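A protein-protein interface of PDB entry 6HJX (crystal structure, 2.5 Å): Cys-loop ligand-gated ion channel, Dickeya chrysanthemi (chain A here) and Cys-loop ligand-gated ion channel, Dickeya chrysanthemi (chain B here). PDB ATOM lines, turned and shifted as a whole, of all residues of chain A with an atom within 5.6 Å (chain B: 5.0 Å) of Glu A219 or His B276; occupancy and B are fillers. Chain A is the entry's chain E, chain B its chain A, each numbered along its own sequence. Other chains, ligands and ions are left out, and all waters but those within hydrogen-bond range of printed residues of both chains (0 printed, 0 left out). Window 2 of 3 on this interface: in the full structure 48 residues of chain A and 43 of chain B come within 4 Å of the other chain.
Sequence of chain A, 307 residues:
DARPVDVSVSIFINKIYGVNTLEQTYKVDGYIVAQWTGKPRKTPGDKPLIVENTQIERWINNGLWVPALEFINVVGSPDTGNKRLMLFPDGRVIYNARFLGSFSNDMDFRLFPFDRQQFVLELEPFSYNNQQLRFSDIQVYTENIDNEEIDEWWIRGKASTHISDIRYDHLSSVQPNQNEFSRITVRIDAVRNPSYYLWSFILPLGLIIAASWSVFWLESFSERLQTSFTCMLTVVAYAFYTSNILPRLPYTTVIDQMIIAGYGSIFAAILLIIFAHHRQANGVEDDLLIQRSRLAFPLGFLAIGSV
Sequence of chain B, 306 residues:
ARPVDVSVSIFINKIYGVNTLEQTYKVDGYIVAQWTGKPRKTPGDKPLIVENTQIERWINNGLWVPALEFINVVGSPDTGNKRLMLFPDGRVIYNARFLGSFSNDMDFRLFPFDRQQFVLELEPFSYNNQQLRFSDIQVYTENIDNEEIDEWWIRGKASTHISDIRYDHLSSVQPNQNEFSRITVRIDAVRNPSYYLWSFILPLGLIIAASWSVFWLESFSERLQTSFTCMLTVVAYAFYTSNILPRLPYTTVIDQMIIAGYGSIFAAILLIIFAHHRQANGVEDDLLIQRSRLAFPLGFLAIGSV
The side-chain carboxylate (OE2) of Glu A219 is in hydrogen-bond range of a ring nitrogen (NE2) of His B276.
Of chain B, only His B276 (2.7 Å) comes within 4 Å of Glu A219.
His B276 touches just one residue of chain A: Glu A219.
Printed residues of chain A within 4 Å of Ile B273: Trp A217.
Of the printed residues of chain A, His B277 touches Trp A217.
Of the printed residues of chain B, Trp A217 touches Phe B220 (3.6 Å), Ile B273 (3.9 Å) and His B277 (3.3 Å).
Of the printed residues of chain A, Phe B220 touches Trp A217 (3.6 Å).
Glu A223 touches none of the printed residues of chain B.
The nearest printed residue of chain A that does not touch His B276 is Trp A217 (5.6 Å).
The nearest printed residue of chain A that does not touch Phe B220 is Glu A219 (4.4 Å).
Among the printed residues, pairs that only touch across the chains: Trp A217 with His B277 (3.3 Å), Trp A217 with Phe B220 (3.6 Å) and Trp A217 with Ile B273 (3.9 Å).
Hydrophobic or aromatic side chains of chain B within 4 Å of the printed part of chain A: Phe B220, Ile B273, His B276 and His B277.
O of Glu A219 is in hydrogen-bond range of NH2 of Arg A224 (3.2 Å).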
ATOM      1  N   TRP A 217      17.935  28.952  28.660  1.00  0.00           N
ATOM      2  CA  TRP A 217      18.638  27.702  28.408  1.00  0.00           C
ATOM      3  C   TRP A 217      18.627  27.297  26.941  1.00  0.00           C
ATOM      4  O   TRP A 217      19.322  26.342  26.575  1.00  0.00           O
ATOM      5  CB  TRP A 217      18.028  26.575  29.253  1.00  0.00           C
ATOM      6  CG  TRP A 217      18.171  26.822  30.716  1.00  0.00           C
ATOM      7  CD1 TRP A 217      17.367  27.598  31.498  1.00  0.00           C
ATOM      8  CD2 TRP A 217      19.191  26.304  31.577  1.00  0.00           C
ATOM      9  NE1 TRP A 217      17.821  27.592  32.795  1.00  0.00           N
ATOM     10  CE2 TRP A 217      18.939  26.805  32.870  1.00  0.00           C
ATOM     11  CE3 TRP A 217      20.291  25.465  31.380  1.00  0.00           C
ATOM     12  CZ2 TRP A 217      19.746  26.492  33.961  1.00  0.00           C
ATOM     13  CZ3 TRP A 217      21.091  25.156  32.465  1.00  0.00           C
ATOM     14  CH2 TRP A 217      20.815  25.668  33.739  1.00  0.00           C
ATOM     15  N   LEU A 218      17.853  27.979  26.103  1.00  0.00           N
ATOM     16  CA  LEU A 218      17.982  27.814  24.663  1.00  0.00           C
ATOM     17  C   LEU A 218      19.264  28.492  24.195  1.00  0.00           C
ATOM     18  O   LEU A 218      19.652  29.545  24.707  1.00  0.00           O
ATOM     19  CB  LEU A 218      16.764  28.399  23.950  1.00  0.00           C
ATOM     20  CG  LEU A 218      15.440  27.695  24.264  1.00  0.00           C
ATOM     21  CD1 LEU A 218      14.263  28.611  23.975  1.00  0.00           C
ATOM     22  CD2 LEU A 218      15.319  26.403  23.470  1.00  0.00           C
ATOM     23  N   GLU A 219      19.927  27.880  23.213  1.00  0.00           N
ATOM     24  CA  GLU A 219      21.300  28.246  22.889  1.00  0.00           C
ATOM     25  C   GLU A 219      21.426  29.262  21.761  1.00  0.00           C
ATOM     26  O   GLU A 219      22.450  29.950  21.689  1.00  0.00           O
ATOM     27  CB  GLU A 219      22.096  26.985  22.537  1.00  0.00           C
ATOM     28  CG  GLU A 219      22.414  26.133  23.759  1.00  0.00           C
ATOM     29  CD  GLU A 219      22.625  24.666  23.431  1.00  0.00           C
ATOM     30  OE1 GLU A 219      22.643  24.311  22.233  1.00  0.00           O
ATOM     31  OE2 GLU A 219      22.769  23.866  24.380  1.00  0.00           O
ATOM     32  N   SER A 220      20.429  29.383  20.891  1.00  0.00           N
ATOM     33  CA  SER A 220      20.451  30.385  19.834  1.00  0.00           C
ATOM     34  C   SER A 220      19.535  31.550  20.192  1.00  0.00           C
ATOM     35  O   SER A 220      18.513  31.378  20.861  1.00  0.00           O
ATOM     36  CB  SER A 220      20.024  29.788  18.493  1.00  0.00           C
ATOM     37  OG  SER A 220      18.614  29.797  18.359  1.00  0.00           O
ATOM     38  N   PHE A 221      19.914  32.744  19.731  1.00  0.00           N
ATOM     39  CA  PHE A 221      19.132  33.939  20.030  1.00  0.00           C
ATOM     40  C   PHE A 221      17.746  33.875  19.400  1.00  0.00           C
ATOM     41  O   PHE A 221      16.761  34.308  20.008  1.00  0.00           O
ATOM     42  CB  PHE A 221      19.882  35.183  19.553  1.00  0.00           C
ATOM     43  CG  PHE A 221      18.989  36.351  19.238  1.00  0.00           C
ATOM     44  CD1 PHE A 221      18.476  37.145  20.250  1.00  0.00           C
ATOM     45  CD2 PHE A 221      18.668  36.657  17.925  1.00  0.00           C
ATOM     46  CE1 PHE A 221      17.655  38.220  19.959  1.00  0.00           C
ATOM     47  CE2 PHE A 221      17.850  37.731  17.628  1.00  0.00           C
ATOM     48  CZ  PHE A 221      17.344  38.514  18.646  1.00  0.00           C
ATOM     49  N   GLU A 223      15.961  31.381  19.088  1.00  0.00           N
ATOM     50  CA  GLU A 223      15.121  30.466  19.852  1.00  0.00           C
ATOM     51  C   GLU A 223      14.623  31.108  21.140  1.00  0.00           C
ATOM     52  O   GLU A 223      13.457  30.934  21.511  1.00  0.00           O
ATOM     53  CB  GLU A 223      15.894  29.184  20.162  1.00  0.00           C
ATOM     54  CG  GLU A 223      16.103  28.290  18.951  1.00  0.00           C
ATOM     55  CD  GLU A 223      17.135  27.207  19.195  1.00  0.00           C
ATOM     56  OE1 GLU A 223      17.595  27.067  20.349  1.00  0.00           O
ATOM     57  OE2 GLU A 223      17.485  26.496  18.229  1.00  0.00           O
ATOM     58  N   ARG A 224      15.486  31.853  21.834  1.00  0.00           N
ATOM     59  CA  ARG A 224      15.078  32.489  23.081  1.00  0.00           C
ATOM     60  C   ARG A 224      13.911  33.441  22.853  1.00  0.00           C
ATOM     61  O   ARG A 224      12.919  33.420  23.590  1.00  0.00           O
ATOM     62  CB  ARG A 224      16.259  33.240  23.700  1.00  0.00           C
ATOM     63  CG  ARG A 224      17.538  32.427  23.816  1.00  0.00           C
ATOM     64  CD  ARG A 224      18.615  33.182  24.587  1.00  0.00           C
ATOM     65  NE  ARG A 224      19.950  32.646  24.322  1.00  0.00           N
ATOM     66  CZ  ARG A 224      20.843  33.195  23.502  1.00  0.00           C
ATOM     67  NH1 ARG A 224      20.574  34.320  22.852  1.00  0.00           N
ATOM     68  NH2 ARG A 224      22.025  32.617  23.336  1.00  0.00           N
ATOM     69  N   LEU A 288      26.962  35.674  25.180  1.00  0.00           N
ATOM     70  CA  LEU A 288      26.384  34.567  25.929  1.00  0.00           C
ATOM     71  C   LEU A 288      26.756  34.613  27.406  1.00  0.00           C
ATOM     72  O   LEU A 288      26.273  33.778  28.178  1.00  0.00           O
ATOM     73  CB  LEU A 288      26.824  33.226  25.330  1.00  0.00           C
ATOM     74  CG  LEU A 288      26.535  32.991  23.843  1.00  0.00           C
ATOM     75  CD1 LEU A 288      26.780  31.531  23.489  1.00  0.00           C
ATOM     76  CD2 LEU A 288      25.118  33.401  23.468  1.00  0.00           C
ATOM     77  N   PHE B 220      17.539  18.770  21.220  1.00  0.00           N
ATOM     78  CA  PHE B 220      17.198  19.413  22.485  1.00  0.00           C
ATOM     79  C   PHE B 220      16.273  20.603  22.263  1.00  0.00           C
ATOM     80  O   PHE B 220      15.294  20.784  22.996  1.00  0.00           O
ATOM     81  CB  PHE B 220      18.469  19.852  23.211  1.00  0.00           C
ATOM     82  CG  PHE B 220      18.252  20.956  24.206  1.00  0.00           C
ATOM     83  CD1 PHE B 220      17.628  20.706  25.414  1.00  0.00           C
ATOM     84  CD2 PHE B 220      18.680  22.244  23.934  1.00  0.00           C
ATOM     85  CE1 PHE B 220      17.430  21.723  26.330  1.00  0.00           C
ATOM     86  CE2 PHE B 220      18.485  23.262  24.848  1.00  0.00           C
ATOM     87  CZ  PHE B 220      17.861  23.002  26.045  1.00  0.00           C
ATOM     88  N   ARG B 223      12.804  19.349  21.472  1.00  0.00           N
ATOM     89  CA  ARG B 223      12.154  18.761  22.639  1.00  0.00           C
ATOM     90  C   ARG B 223      11.614  19.835  23.576  1.00  0.00           C
ATOM     91  O   ARG B 223      10.504  19.706  24.106  1.00  0.00           O
ATOM     92  CB  ARG B 223      13.136  17.853  23.382  1.00  0.00           C
ATOM     93  CG  ARG B 223      13.455  16.551  22.671  1.00  0.00           C
ATOM     94  CD  ARG B 223      14.291  15.628  23.547  1.00  0.00           C
ATOM     95  NE  ARG B 223      15.642  16.140  23.769  1.00  0.00           N
ATOM     96  CZ  ARG B 223      16.708  15.801  23.047  1.00  0.00           C
ATOM     97  NH1 ARG B 223      16.601  14.942  22.040  1.00  0.00           N
ATOM     98  NH2 ARG B 223      17.889  16.328  23.335  1.00  0.00           N
ATOM     99  N   ILE B 272      14.269  17.460  30.191  1.00  0.00           N
ATOM    100  CA  ILE B 272      14.896  17.737  28.901  1.00  0.00           C
ATOM    101  C   ILE B 272      16.064  18.698  29.066  1.00  0.00           C
ATOM    102  O   ILE B 272      17.058  18.612  28.333  1.00  0.00           O
ATOM    103  CB  ILE B 272      13.840  18.283  27.915  1.00  0.00           C
ATOM    104  CG1 ILE B 272      12.880  17.163  27.503  1.00  0.00           C
ATOM    105  CG2 ILE B 272      14.500  18.899  26.685  1.00  0.00           C
ATOM    106  CD1 ILE B 272      11.577  17.656  26.910  1.00  0.00           C
ATOM    107  N   ILE B 273      15.972  19.619  30.026  1.00  0.00           N
ATOM    108  CA  ILE B 273      17.050  20.573  30.261  1.00  0.00           C
ATOM    109  C   ILE B 273      18.152  19.949  31.108  1.00  0.00           C
ATOM    110  O   ILE B 273      19.341  20.195  30.873  1.00  0.00           O
ATOM    111  CB  ILE B 273      16.480  21.847  30.909  1.00  0.00           C
ATOM    112  CG1 ILE B 273      15.674  22.636  29.875  1.00  0.00           C
ATOM    113  CG2 ILE B 273      17.592  22.710  31.500  1.00  0.00           C
ATOM    114  CD1 ILE B 273      14.825  23.740  30.465  1.00  0.00           C
ATOM    115  N   PHE B 274      17.782  19.147  32.109  1.00  0.00           N
ATOM    116  CA  PHE B 274      18.784  18.463  32.920  1.00  0.00           C
ATOM    117  C   PHE B 274      19.667  17.569  32.059  1.00  0.00           C
ATOM    118  O   PHE B 274      20.895  17.569  32.206  1.00  0.00           O
ATOM    119  CB  PHE B 274      18.094  17.647  34.015  1.00  0.00           C
ATOM    120  CG  PHE B 274      19.027  16.784  34.819  1.00  0.00           C
ATOM    121  CD1 PHE B 274      19.934  17.349  35.700  1.00  0.00           C
ATOM    122  CD2 PHE B 274      18.982  15.404  34.706  1.00  0.00           C
ATOM    123  CE1 PHE B 274      20.788  16.554  36.447  1.00  0.00           C
ATOM    124  CE2 PHE B 274      19.831  14.604  35.451  1.00  0.00           C
ATOM    125  CZ  PHE B 274      20.735  15.180  36.322  1.00  0.00           C
ATOM    126  N   ALA B 275      19.061  16.820  31.141  1.00  0.00           N
ATOM    127  CA  ALA B 275      19.767  15.904  30.247  1.00  0.00           C
ATOM    128  C   ALA B 275      20.604  16.612  29.199  1.00  0.00           C
ATOM    129  O   ALA B 275      21.117  15.924  28.307  1.00  0.00           O
ATOM    130  CB  ALA B 275      18.756  14.986  29.555  1.00  0.00           C
ATOM    131  N   HIS B 276      20.766  17.934  29.269  1.00  0.00           N
ATOM    132  CA  HIS B 276      21.502  18.679  28.256  1.00  0.00           C
ATOM    133  C   HIS B 276      22.542  19.633  28.824  1.00  0.00           C
ATOM    134  O   HIS B 276      23.454  20.023  28.084  1.00  0.00           O
ATOM    135  CB  HIS B 276      20.530  19.484  27.378  1.00  0.00           C
ATOM    136  CG  HIS B 276      21.155  20.042  26.138  1.00  0.00           C
ATOM    137  ND1 HIS B 276      21.439  19.266  25.035  1.00  0.00           N
ATOM    138  CD2 HIS B 276      21.546  21.301  25.825  1.00  0.00           C
ATOM    139  CE1 HIS B 276      21.981  20.021  24.097  1.00  0.00           C
ATOM    140  NE2 HIS B 276      22.056  21.259  24.550  1.00  0.00           N
ATOM    141  N   HIS B 277      22.446  20.021  30.097  1.00  0.00           N
ATOM    142  CA  HIS B 277      23.385  20.957  30.706  1.00  0.00           C
ATOM    143  C   HIS B 277      24.065  20.383  31.943  1.00  0.00           C
ATOM    144  O   HIS B 277      24.740  21.127  32.666  1.00  0.00           O
ATOM    145  CB  HIS B 277      22.676  22.265  31.073  1.00  0.00           C
ATOM    146  CG  HIS B 277      22.454  23.185  29.913  1.00  0.00           C
ATOM    147  ND1 HIS B 277      21.299  23.172  29.162  1.00  0.00           N
ATOM    148  CD2 HIS B 277      23.238  24.151  29.381  1.00  0.00           C
ATOM    149  CE1 HIS B 277      21.382  24.090  28.214  1.00  0.00           C
ATOM    150  NE2 HIS B 277      22.550  24.698  28.325  1.00  0.00           N
ATOM    151  N   ARG B 278      23.909  19.079  32.211  1.00  0.00           N
ATOM    152  CA  ARG B 278      24.499  18.442  33.392  1.00  0.00           C
ATOM    153  C   ARG B 278      25.027  17.072  32.962  1.00  0.00           C
ATOM    154  O   ARG B 278      24.406  16.034  33.207  1.00  0.00           O
ATOM    155  CB  ARG B 278      23.489  18.327  34.531  1.00  0.00           C
ATOM    156  N   GLU B 284      27.812  17.733  26.059  1.00  0.00           N
ATOM    157  CA  GLU B 284      27.644  16.295  26.241  1.00  0.00           C
ATOM    158  C   GLU B 284      26.182  15.954  26.511  1.00  0.00           C
ATOM    159  O   GLU B 284      25.768  15.818  27.662  1.00  0.00           O
ATOM    160  CB  GLU B 284      28.522  15.795  27.391  1.00  0.00           C
ATOM    161  N   ASP B 285      25.404  15.815  25.439  1.00  0.00           N
ATOM    162  CA  ASP B 285      23.984  15.524  25.576  1.00  0.00           C
ATOM    163  C   ASP B 285      23.769  14.101  26.075  1.00  0.00           C
ATOM    164  O   ASP B 285      24.421  13.158  25.619  1.00  0.00           O
ATOM    165  CB  ASP B 285      23.270  15.723  24.239  1.00  0.00           C
